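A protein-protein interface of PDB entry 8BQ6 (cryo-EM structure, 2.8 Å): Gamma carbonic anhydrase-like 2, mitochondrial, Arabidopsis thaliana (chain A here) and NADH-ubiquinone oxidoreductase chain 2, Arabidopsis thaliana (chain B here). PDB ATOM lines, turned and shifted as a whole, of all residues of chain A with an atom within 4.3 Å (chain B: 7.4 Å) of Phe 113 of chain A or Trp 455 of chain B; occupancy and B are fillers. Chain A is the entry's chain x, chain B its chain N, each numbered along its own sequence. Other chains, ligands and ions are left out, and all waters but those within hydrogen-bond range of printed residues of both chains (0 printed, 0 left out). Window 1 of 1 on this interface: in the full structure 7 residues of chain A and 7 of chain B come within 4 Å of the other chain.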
ATOM      1  N   TRP A  91     -10.550  18.287   4.973  1.00  0.00           N
ATOM      2  CA  TRP A  91     -11.280  19.131   5.902  1.00  0.00           C
ATOM      3  C   TRP A  91     -11.011  18.727   7.350  1.00  0.00           C
ATOM      4  O   TRP A  91     -10.240  17.811   7.643  1.00  0.00           O
ATOM      5  CB  TRP A  91     -12.773  19.092   5.588  1.00  0.00           C
ATOM      6  CG  TRP A  91     -13.132  19.974   4.449  1.00  0.00           C
ATOM      7  CD1 TRP A  91     -13.388  19.588   3.172  1.00  0.00           C
ATOM      8  CD2 TRP A  91     -13.258  21.399   4.471  1.00  0.00           C
ATOM      9  NE1 TRP A  91     -13.670  20.680   2.394  1.00  0.00           N
ATOM     10  CE2 TRP A  91     -13.598  21.806   3.169  1.00  0.00           C
ATOM     11  CE3 TRP A  91     -13.122  22.369   5.468  1.00  0.00           C
ATOM     12  CZ2 TRP A  91     -13.807  23.139   2.837  1.00  0.00           C
ATOM     13  CZ3 TRP A  91     -13.330  23.689   5.136  1.00  0.00           C
ATOM     14  CH2 TRP A  91     -13.667  24.063   3.832  1.00  0.00           C
ATOM     15  N   ASP A  92     -11.671  19.432   8.265  1.00  0.00           N
ATOM     16  CA  ASP A  92     -11.401  19.291   9.689  1.00  0.00           C
ATOM     17  C   ASP A  92     -11.729  17.887  10.180  1.00  0.00           C
ATOM     18  O   ASP A  92     -12.770  17.319   9.841  1.00  0.00           O
ATOM     19  CB  ASP A  92     -12.217  20.317  10.469  1.00  0.00           C
ATOM     20  CG  ASP A  92     -12.035  21.725   9.940  1.00  0.00           C
ATOM     21  OD1 ASP A  92     -11.233  22.485  10.516  1.00  0.00           O
ATOM     22  OD2 ASP A  92     -12.687  22.067   8.932  1.00  0.00           O
ATOM     23  N   GLY A 112     -14.244  15.027   3.435  1.00  0.00           N
ATOM     24  CA  GLY A 112     -15.158  15.777   4.266  1.00  0.00           C
ATOM     25  C   GLY A 112     -14.865  15.702   5.750  1.00  0.00           C
ATOM     26  O   GLY A 112     -13.881  15.122   6.207  1.00  0.00           O
ATOM     27  N   PHE A 113     -15.765  16.314   6.515  1.00  0.00           N
ATOM     28  CA  PHE A 113     -15.600  16.416   7.957  1.00  0.00           C
ATOM     29  C   PHE A 113     -15.583  15.035   8.602  1.00  0.00           C
ATOM     30  O   PHE A 113     -16.519  14.248   8.434  1.00  0.00           O
ATOM     31  CB  PHE A 113     -16.728  17.267   8.538  1.00  0.00           C
ATOM     32  CG  PHE A 113     -16.734  17.326  10.033  1.00  0.00           C
ATOM     33  CD1 PHE A 113     -15.791  18.069  10.711  1.00  0.00           C
ATOM     34  CD2 PHE A 113     -17.684  16.634  10.760  1.00  0.00           C
ATOM     35  CE1 PHE A 113     -15.794  18.125  12.079  1.00  0.00           C
ATOM     36  CE2 PHE A 113     -17.690  16.687  12.133  1.00  0.00           C
ATOM     37  CZ  PHE A 113     -16.745  17.432  12.793  1.00  0.00           C
ATOM     38  N   CYS A 114     -14.510  14.746   9.343  1.00  0.00           N
ATOM     39  CA  CYS A 114     -14.319  13.462  10.023  1.00  0.00           C
ATOM     40  C   CYS A 114     -14.422  12.275   9.073  1.00  0.00           C
ATOM     41  O   CYS A 114     -14.960  11.227   9.433  1.00  0.00           O
ATOM     42  CB  CYS A 114     -15.303  13.280  11.181  1.00  0.00           C
ATOM     43  SG  CYS A 114     -15.080  11.764  12.123  1.00  0.00           S
ATOM     44  N   SER A 115     -13.911  12.418   7.861  1.00  0.00           N
ATOM     45  CA  SER A 115     -13.863  11.316   6.917  1.00  0.00           C
ATOM     46  C   SER A 115     -12.445  10.770   6.854  1.00  0.00           C
ATOM     47  O   SER A 115     -11.475  11.467   7.140  1.00  0.00           O
ATOM     48  CB  SER A 115     -14.331  11.769   5.536  1.00  0.00           C
ATOM     49  OG  SER A 115     -15.736  11.655   5.432  1.00  0.00           O
ATOM     50  N   ARG A 141     -19.063  13.866   4.758  1.00  0.00           N
ATOM     51  CA  ARG A 141     -18.706  13.747   6.163  1.00  0.00           C
ATOM     52  C   ARG A 141     -19.048  12.368   6.716  1.00  0.00           C
ATOM     53  O   ARG A 141     -19.981  11.701   6.261  1.00  0.00           O
ATOM     54  CB  ARG A 141     -19.424  14.816   6.977  1.00  0.00           C
ATOM     55  CG  ARG A 141     -20.920  14.649   6.979  1.00  0.00           C
ATOM     56  CD  ARG A 141     -21.561  15.624   7.921  1.00  0.00           C
ATOM     57  NE  ARG A 141     -23.004  15.439   7.989  1.00  0.00           N
ATOM     58  CZ  ARG A 141     -23.865  15.927   7.107  1.00  0.00           C
ATOM     59  NH1 ARG A 141     -23.462  16.636   6.066  1.00  0.00           N
ATOM     60  NH2 ARG A 141     -25.164  15.702   7.277  1.00  0.00           N
ATOM     61  N   TYR A 142     -18.281  11.953   7.724  1.00  0.00           N
ATOM     62  CA  TYR A 142     -18.481  10.673   8.406  1.00  0.00           C
ATOM     63  C   TYR A 142     -18.430   9.498   7.434  1.00  0.00           C
ATOM     64  O   TYR A 142     -19.182   8.532   7.563  1.00  0.00           O
ATOM     65  CB  TYR A 142     -19.803  10.648   9.178  1.00  0.00           C
ATOM     66  CG  TYR A 142     -19.910  11.645  10.298  1.00  0.00           C
ATOM     67  CD1 TYR A 142     -18.995  11.648  11.337  1.00  0.00           C
ATOM     68  CD2 TYR A 142     -20.945  12.567  10.332  1.00  0.00           C
ATOM     69  CE1 TYR A 142     -19.093  12.551  12.364  1.00  0.00           C
ATOM     70  CE2 TYR A 142     -21.053  13.475  11.358  1.00  0.00           C
ATOM     71  CZ  TYR A 142     -20.124  13.461  12.371  1.00  0.00           C
ATOM     72  OH  TYR A 142     -20.219  14.363  13.399  1.00  0.00           O
ATOM     73  N   ASP B 376     -26.929  29.295   8.828  1.00  0.00           N
ATOM     74  CA  ASP B 376     -25.536  28.921   8.461  1.00  0.00           C
ATOM     75  C   ASP B 376     -24.793  28.369   9.683  1.00  0.00           C
ATOM     76  O   ASP B 376     -23.809  27.645   9.482  1.00  0.00           O
ATOM     77  CB  ASP B 376     -24.805  30.111   7.841  1.00  0.00           C
ATOM     78  CG  ASP B 376     -25.381  30.591   6.519  1.00  0.00           C
ATOM     79  OD1 ASP B 376     -26.340  29.962   6.027  1.00  0.00           O
ATOM     80  OD2 ASP B 376     -24.860  31.593   5.986  1.00  0.00           O
ATOM     81  N   GLY B 378     -25.695  26.082  11.586  1.00  0.00           N
ATOM     82  CA  GLY B 378     -26.117  24.729  11.902  1.00  0.00           C
ATOM     83  C   GLY B 378     -24.932  23.791  12.058  1.00  0.00           C
ATOM     84  O   GLY B 378     -23.976  23.828  11.281  1.00  0.00           O
ATOM     85  N   ALA B 379     -25.008  22.942  13.083  1.00  0.00           N
ATOM     86  CA  ALA B 379     -23.981  21.956  13.417  1.00  0.00           C
ATOM     87  C   ALA B 379     -22.628  22.587  13.722  1.00  0.00           C
ATOM     88  O   ALA B 379     -21.589  21.971  13.473  1.00  0.00           O
ATOM     89  CB  ALA B 379     -23.827  20.907  12.309  1.00  0.00           C
ATOM     90  N   LEU B 380     -22.602  23.802  14.271  1.00  0.00           N
ATOM     91  CA  LEU B 380     -21.320  24.392  14.639  1.00  0.00           C
ATOM     92  C   LEU B 380     -20.768  23.768  15.913  1.00  0.00           C
ATOM     93  O   LEU B 380     -19.560  23.831  16.165  1.00  0.00           O
ATOM     94  CB  LEU B 380     -21.459  25.907  14.793  1.00  0.00           C
ATOM     95  CG  LEU B 380     -20.194  26.712  15.102  1.00  0.00           C
ATOM     96  CD1 LEU B 380     -19.215  26.657  13.939  1.00  0.00           C
ATOM     97  CD2 LEU B 380     -20.549  28.145  15.430  1.00  0.00           C
ATOM     98  N   ALA B 381     -21.628  23.145  16.719  1.00  0.00           N
ATOM     99  CA  ALA B 381     -21.147  22.487  17.926  1.00  0.00           C
ATOM    100  C   ALA B 381     -20.417  21.188  17.616  1.00  0.00           C
ATOM    101  O   ALA B 381     -19.696  20.674  18.478  1.00  0.00           O
ATOM    102  CB  ALA B 381     -22.312  22.237  18.879  1.00  0.00           C
ATOM    103  N   LYS B 382     -20.584  20.648  16.410  1.00  0.00           N
ATOM    104  CA  LYS B 382     -19.791  19.510  15.965  1.00  0.00           C
ATOM    105  C   LYS B 382     -18.499  19.948  15.291  1.00  0.00           C
ATOM    106  O   LYS B 382     -17.426  19.426  15.606  1.00  0.00           O
ATOM    107  CB  LYS B 382     -20.592  18.647  14.993  1.00  0.00           C
ATOM    108  CG  LYS B 382     -21.882  18.122  15.554  1.00  0.00           C
ATOM    109  CD  LYS B 382     -21.688  16.735  16.097  1.00  0.00           C
ATOM    110  CE  LYS B 382     -22.158  16.657  17.533  1.00  0.00           C
ATOM    111  NZ  LYS B 382     -21.497  15.552  18.276  1.00  0.00           N
ATOM    112  N   THR B 383     -18.590  20.899  14.364  1.00  0.00           N
ATOM    113  CA  THR B 383     -17.427  21.326  13.601  1.00  0.00           C
ATOM    114  C   THR B 383     -16.452  22.168  14.416  1.00  0.00           C
ATOM    115  O   THR B 383     -15.250  22.127  14.143  1.00  0.00           O
ATOM    116  CB  THR B 383     -17.883  22.083  12.349  1.00  0.00           C
ATOM    117  OG1 THR B 383     -18.535  23.300  12.729  1.00  0.00           O
ATOM    118  CG2 THR B 383     -18.837  21.231  11.535  1.00  0.00           C
ATOM    119  N   ASN B 384     -16.929  22.905  15.414  1.00  0.00           N
ATOM    120  CA  ASN B 384     -16.051  23.706  16.260  1.00  0.00           C
ATOM    121  C   ASN B 384     -16.703  23.868  17.626  1.00  0.00           C
ATOM    122  O   ASN B 384     -17.257  24.932  17.930  1.00  0.00           O
ATOM    123  CB  ASN B 384     -15.774  25.067  15.615  1.00  0.00           C
ATOM    124  CG  ASN B 384     -14.541  25.753  16.184  1.00  0.00           C
ATOM    125  OD1 ASN B 384     -14.070  25.420  17.270  1.00  0.00           O
ATOM    126  ND2 ASN B 384     -14.018  26.725  15.447  1.00  0.00           N
ATOM    127  N   PRO B 385     -16.663  22.832  18.470  1.00  0.00           N
ATOM    128  CA  PRO B 385     -17.422  22.889  19.736  1.00  0.00           C
ATOM    129  C   PRO B 385     -17.047  24.042  20.655  1.00  0.00           C
ATOM    130  O   PRO B 385     -17.939  24.636  21.272  1.00  0.00           O
ATOM    131  CB  PRO B 385     -17.136  21.519  20.374  1.00  0.00           C
ATOM    132  CG  PRO B 385     -16.533  20.681  19.292  1.00  0.00           C
ATOM    133  CD  PRO B 385     -15.872  21.600  18.339  1.00  0.00           C
ATOM    134  N   ASP B 450     -29.881  21.313  16.076  1.00  0.00           N
ATOM    135  CA  ASP B 450     -30.316  21.026  14.719  1.00  0.00           C
ATOM    136  C   ASP B 450     -29.401  20.001  14.063  1.00  0.00           C
ATOM    137  O   ASP B 450     -28.213  19.901  14.380  1.00  0.00           O
ATOM    138  CB  ASP B 450     -30.342  22.306  13.890  1.00  0.00           C
ATOM    139  CG  ASP B 450     -31.664  23.028  13.985  1.00  0.00           C
ATOM    140  OD1 ASP B 450     -32.718  22.364  13.908  1.00  0.00           O
ATOM    141  OD2 ASP B 450     -31.650  24.264  14.144  1.00  0.00           O
ATOM    142  N   THR B 451     -29.969  19.237  13.133  1.00  0.00           N
ATOM    143  CA  THR B 451     -29.223  18.258  12.342  1.00  0.00           C
ATOM    144  C   THR B 451     -29.463  18.547  10.867  1.00  0.00           C
ATOM    145  O   THR B 451     -30.284  17.889  10.215  1.00  0.00           O
ATOM    146  CB  THR B 451     -29.615  16.821  12.700  1.00  0.00           C
ATOM    147  OG1 THR B 451     -31.042  16.685  12.699  1.00  0.00           O
ATOM    148  CG2 THR B 451     -29.064  16.433  14.062  1.00  0.00           C
ATOM    149  N   PRO B 452     -28.753  19.524  10.306  1.00  0.00           N
ATOM    150  CA  PRO B 452     -28.959  19.873   8.899  1.00  0.00           C
ATOM    151  C   PRO B 452     -28.382  18.824   7.963  1.00  0.00           C
ATOM    152  O   PRO B 452     -27.469  18.068   8.304  1.00  0.00           O
ATOM    153  CB  PRO B 452     -28.224  21.209   8.740  1.00  0.00           C
ATOM    154  CG  PRO B 452     -27.404  21.387   9.972  1.00  0.00           C
ATOM    155  CD  PRO B 452     -27.605  20.230  10.893  1.00  0.00           C
ATOM    156  N   ARG B 453     -28.936  18.796   6.752  1.00  0.00           N
ATOM    157  CA  ARG B 453     -28.397  17.918   5.723  1.00  0.00           C
ATOM    158  C   ARG B 453     -27.065  18.438   5.193  1.00  0.00           C
ATOM    159  O   ARG B 453     -26.129  17.658   4.984  1.00  0.00           O
ATOM    160  CB  ARG B 453     -29.418  17.757   4.597  1.00  0.00           C
ATOM    161  CG  ARG B 453     -28.853  17.141   3.339  1.00  0.00           C
ATOM    162  CD  ARG B 453     -28.633  15.650   3.494  1.00  0.00           C
ATOM    163  NE  ARG B 453     -28.143  15.055   2.257  1.00  0.00           N
ATOM    164  CZ  ARG B 453     -26.870  15.053   1.889  1.00  0.00           C
ATOM    165  NH1 ARG B 453     -25.940  15.648   2.619  1.00  0.00           N
ATOM    166  NH2 ARG B 453     -26.521  14.447   0.758  1.00  0.00           N
ATOM    167  N   THR B 454     -26.950  19.747   4.987  1.00  0.00           N
ATOM    168  CA  THR B 454     -25.735  20.353   4.460  1.00  0.00           C
ATOM    169  C   THR B 454     -25.091  21.194   5.555  1.00  0.00           C
ATOM    170  O   THR B 454     -25.766  22.013   6.188  1.00  0.00           O
ATOM    171  CB  THR B 454     -26.045  21.207   3.225  1.00  0.00           C
ATOM    172  OG1 THR B 454     -26.415  20.349   2.140  1.00  0.00           O
ATOM    173  CG2 THR B 454     -24.823  22.004   2.793  1.00  0.00           C
ATOM    174  N   TRP B 455     -23.802  20.972   5.796  1.00  0.00           N
ATOM    175  CA  TRP B 455     -23.039  21.722   6.784  1.00  0.00           C
ATOM    176  C   TRP B 455     -22.120  22.720   6.091  1.00  0.00           C
ATOM    177  O   TRP B 455     -21.670  22.500   4.965  1.00  0.00           O
ATOM    178  CB  TRP B 455     -22.191  20.795   7.666  1.00  0.00           C
ATOM    179  CG  TRP B 455     -22.946  19.794   8.498  1.00  0.00           C
ATOM    180  CD1 TRP B 455     -24.274  19.506   8.435  1.00  0.00           C
ATOM    181  CD2 TRP B 455     -22.400  18.941   9.516  1.00  0.00           C
ATOM    182  NE1 TRP B 455     -24.592  18.532   9.349  1.00  0.00           N
ATOM    183  CE2 TRP B 455     -23.459  18.169  10.025  1.00  0.00           C
ATOM    184  CE3 TRP B 455     -21.119  18.759  10.043  1.00  0.00           C
ATOM    185  CZ2 TRP B 455     -23.279  17.229  11.036  1.00  0.00           C
ATOM    186  CZ3 TRP B 455     -20.942  17.827  11.048  1.00  0.00           C
ATOM    187  CH2 TRP B 455     -22.016  17.075  11.535  1.00  0.00           C
ATOM    188  N   ILE B 456     -21.837  23.821   6.780  1.00  0.00           N
ATOM    189  CA  ILE B 456     -20.816  24.772   6.357  1.00  0.00           C
ATOM    190  C   ILE B 456     -19.634  24.622   7.298  1.00  0.00           C
ATOM    191  O   ILE B 456     -19.779  24.767   8.517  1.00  0.00           O
ATOM    192  CB  ILE B 456     -21.340  26.216   6.354  1.00  0.00           C
ATOM    193  CG1 ILE B 456     -22.261  26.441   5.156  1.00  0.00           C
ATOM    194  CG2 ILE B 456     -20.185  27.208   6.341  1.00  0.00           C
ATOM    195  CD1 ILE B 456     -23.254  27.539   5.366  1.00  0.00           C
ATOM    196  N   LEU B 457     -18.467  24.320   6.740  1.00  0.00           N
ATOM    197  CA  LEU B 457     -17.250  24.221   7.531  1.00  0.00           C
ATOM    198  C   LEU B 457     -16.545  25.570   7.501  1.00  0.00           C
ATOM    199  O   LEU B 457     -16.342  26.150   6.429  1.00  0.00           O
ATOM    200  CB  LEU B 457     -16.345  23.103   7.014  1.00  0.00           C
ATOM    201  CG  LEU B 457     -17.036  21.753   6.806  1.00  0.00           C
ATOM    202  CD1 LEU B 457     -16.041  20.680   6.395  1.00  0.00           C
ATOM    203  CD2 LEU B 457     -17.774  21.336   8.060  1.00  0.00           C
ATOM    204  N   TYR B 458     -16.196  26.074   8.678  1.00  0.00           N
ATOM    205  CA  TYR B 458     -15.657  27.415   8.825  1.00  0.00           C
ATOM    206  C   TYR B 458     -14.156  27.353   9.056  1.00  0.00           C
ATOM    207  O   TYR B 458     -13.656  26.447   9.728  1.00  0.00           O
ATOM    208  CB  TYR B 458     -16.333  28.150   9.983  1.00  0.00           C
ATOM    209  CG  TYR B 458     -17.786  28.458   9.726  1.00  0.00           C
ATOM    210  CD1 TYR B 458     -18.154  29.603   9.042  1.00  0.00           C
ATOM    211  CD2 TYR B 458     -18.792  27.610  10.179  1.00  0.00           C
ATOM    212  CE1 TYR B 458     -19.471  29.891   8.798  1.00  0.00           C
ATOM    213  CE2 TYR B 458     -20.120  27.896   9.942  1.00  0.00           C
ATOM    214  CZ  TYR B 458     -20.450  29.040   9.250  1.00  0.00           C
ATOM    215  OH  TYR B 458     -21.765  29.349   9.002  1.00  0.00           O
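N of Tyr 142 of chain A sits at hydrogen-bond distance from OG of Ser 115 of chain A (3.4 Å).
O of Ala 379 of chain B sits at hydrogen-bond distance from OG1 of Thr 383 of chain B (3.4 Å).
The backbone carbonyl oxygen (O) of Phe 113 of chain A sits at hydrogen-bond distance from the backbone NH (N) of Tyr 142 of chain A, 3.0 Å away.
The backbone carbonyl oxygen (O) of Pro 452 of chain B is in hydrogen-bond range of the indole nitrogen (NE1) of Trp 455 of chain B (3.1 Å).
Among the printed residues, merely in contact across the chains: Trp 91 of chain A with Leu 457 of chain B (3.5 Å), Phe 113 of chain A with Lys 382 of chain B (3.5 Å), Phe 113 of chain A with Thr 383 of chain B (3.9 Å), Phe 113 of chain A with Trp 455 of chain B (3.5 Å), Arg 141 of chain A with Trp 455 of chain B (3.4 Å), Tyr 142 of chain A with Lys 382 of chain B (3.9 Å) and Tyr 142 of chain A with Trp 455 of chain B (3.7 Å).
The guanidinium group (NH2) of Arg 141 of chain A lies within hydrogen-bond range of the backbone carbonyl oxygen (O) of Pro 452 of chain B.
O of Arg 453 of chain B sits at hydrogen-bond distance from NH1 of Arg 141 of chain A (3.1 Å).
Phe 113 of chain A touches just these residues of chain B: Lys 382 (3.5 Å), Thr 383 (3.9 Å) and Trp 455 (3.5 Å).
Of the printed residues of chain B, Tyr 142 of chain A touches Lys 382 (3.9 Å) and Trp 455 (3.7 Å).
Printed residues of chain A within 4 Å of Trp 455 of chain B: Phe 113, Arg 141 and Tyr 142.
Printed residues of chain A within 4 Å of Leu 457 of chain B: Trp 91 (3.5 Å).
Tyr 458 of chain B touches none of the printed residues of chain A.
The nearest residue of chain B that does not touch Phe 113 of chain A is Leu 457 of chain B (4.1 Å).
Of the 18 printed residues of chain B, 6 touch a printed residue of chain A.
Along chain B the printed residues that touch a printed residue of chain A span positions 382 to 457.
Hydrophobic or aromatic side chains of chain A that line the printed part of chain B: Trp 91, Phe 113 and Tyr 142.
Among the printed residues, 9 pairs touch across the chains.
Among the printed residues, no Asp or Glu carboxylate lies within 4 Å of a Lys or Arg side-chain nitrogen of the other chain.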
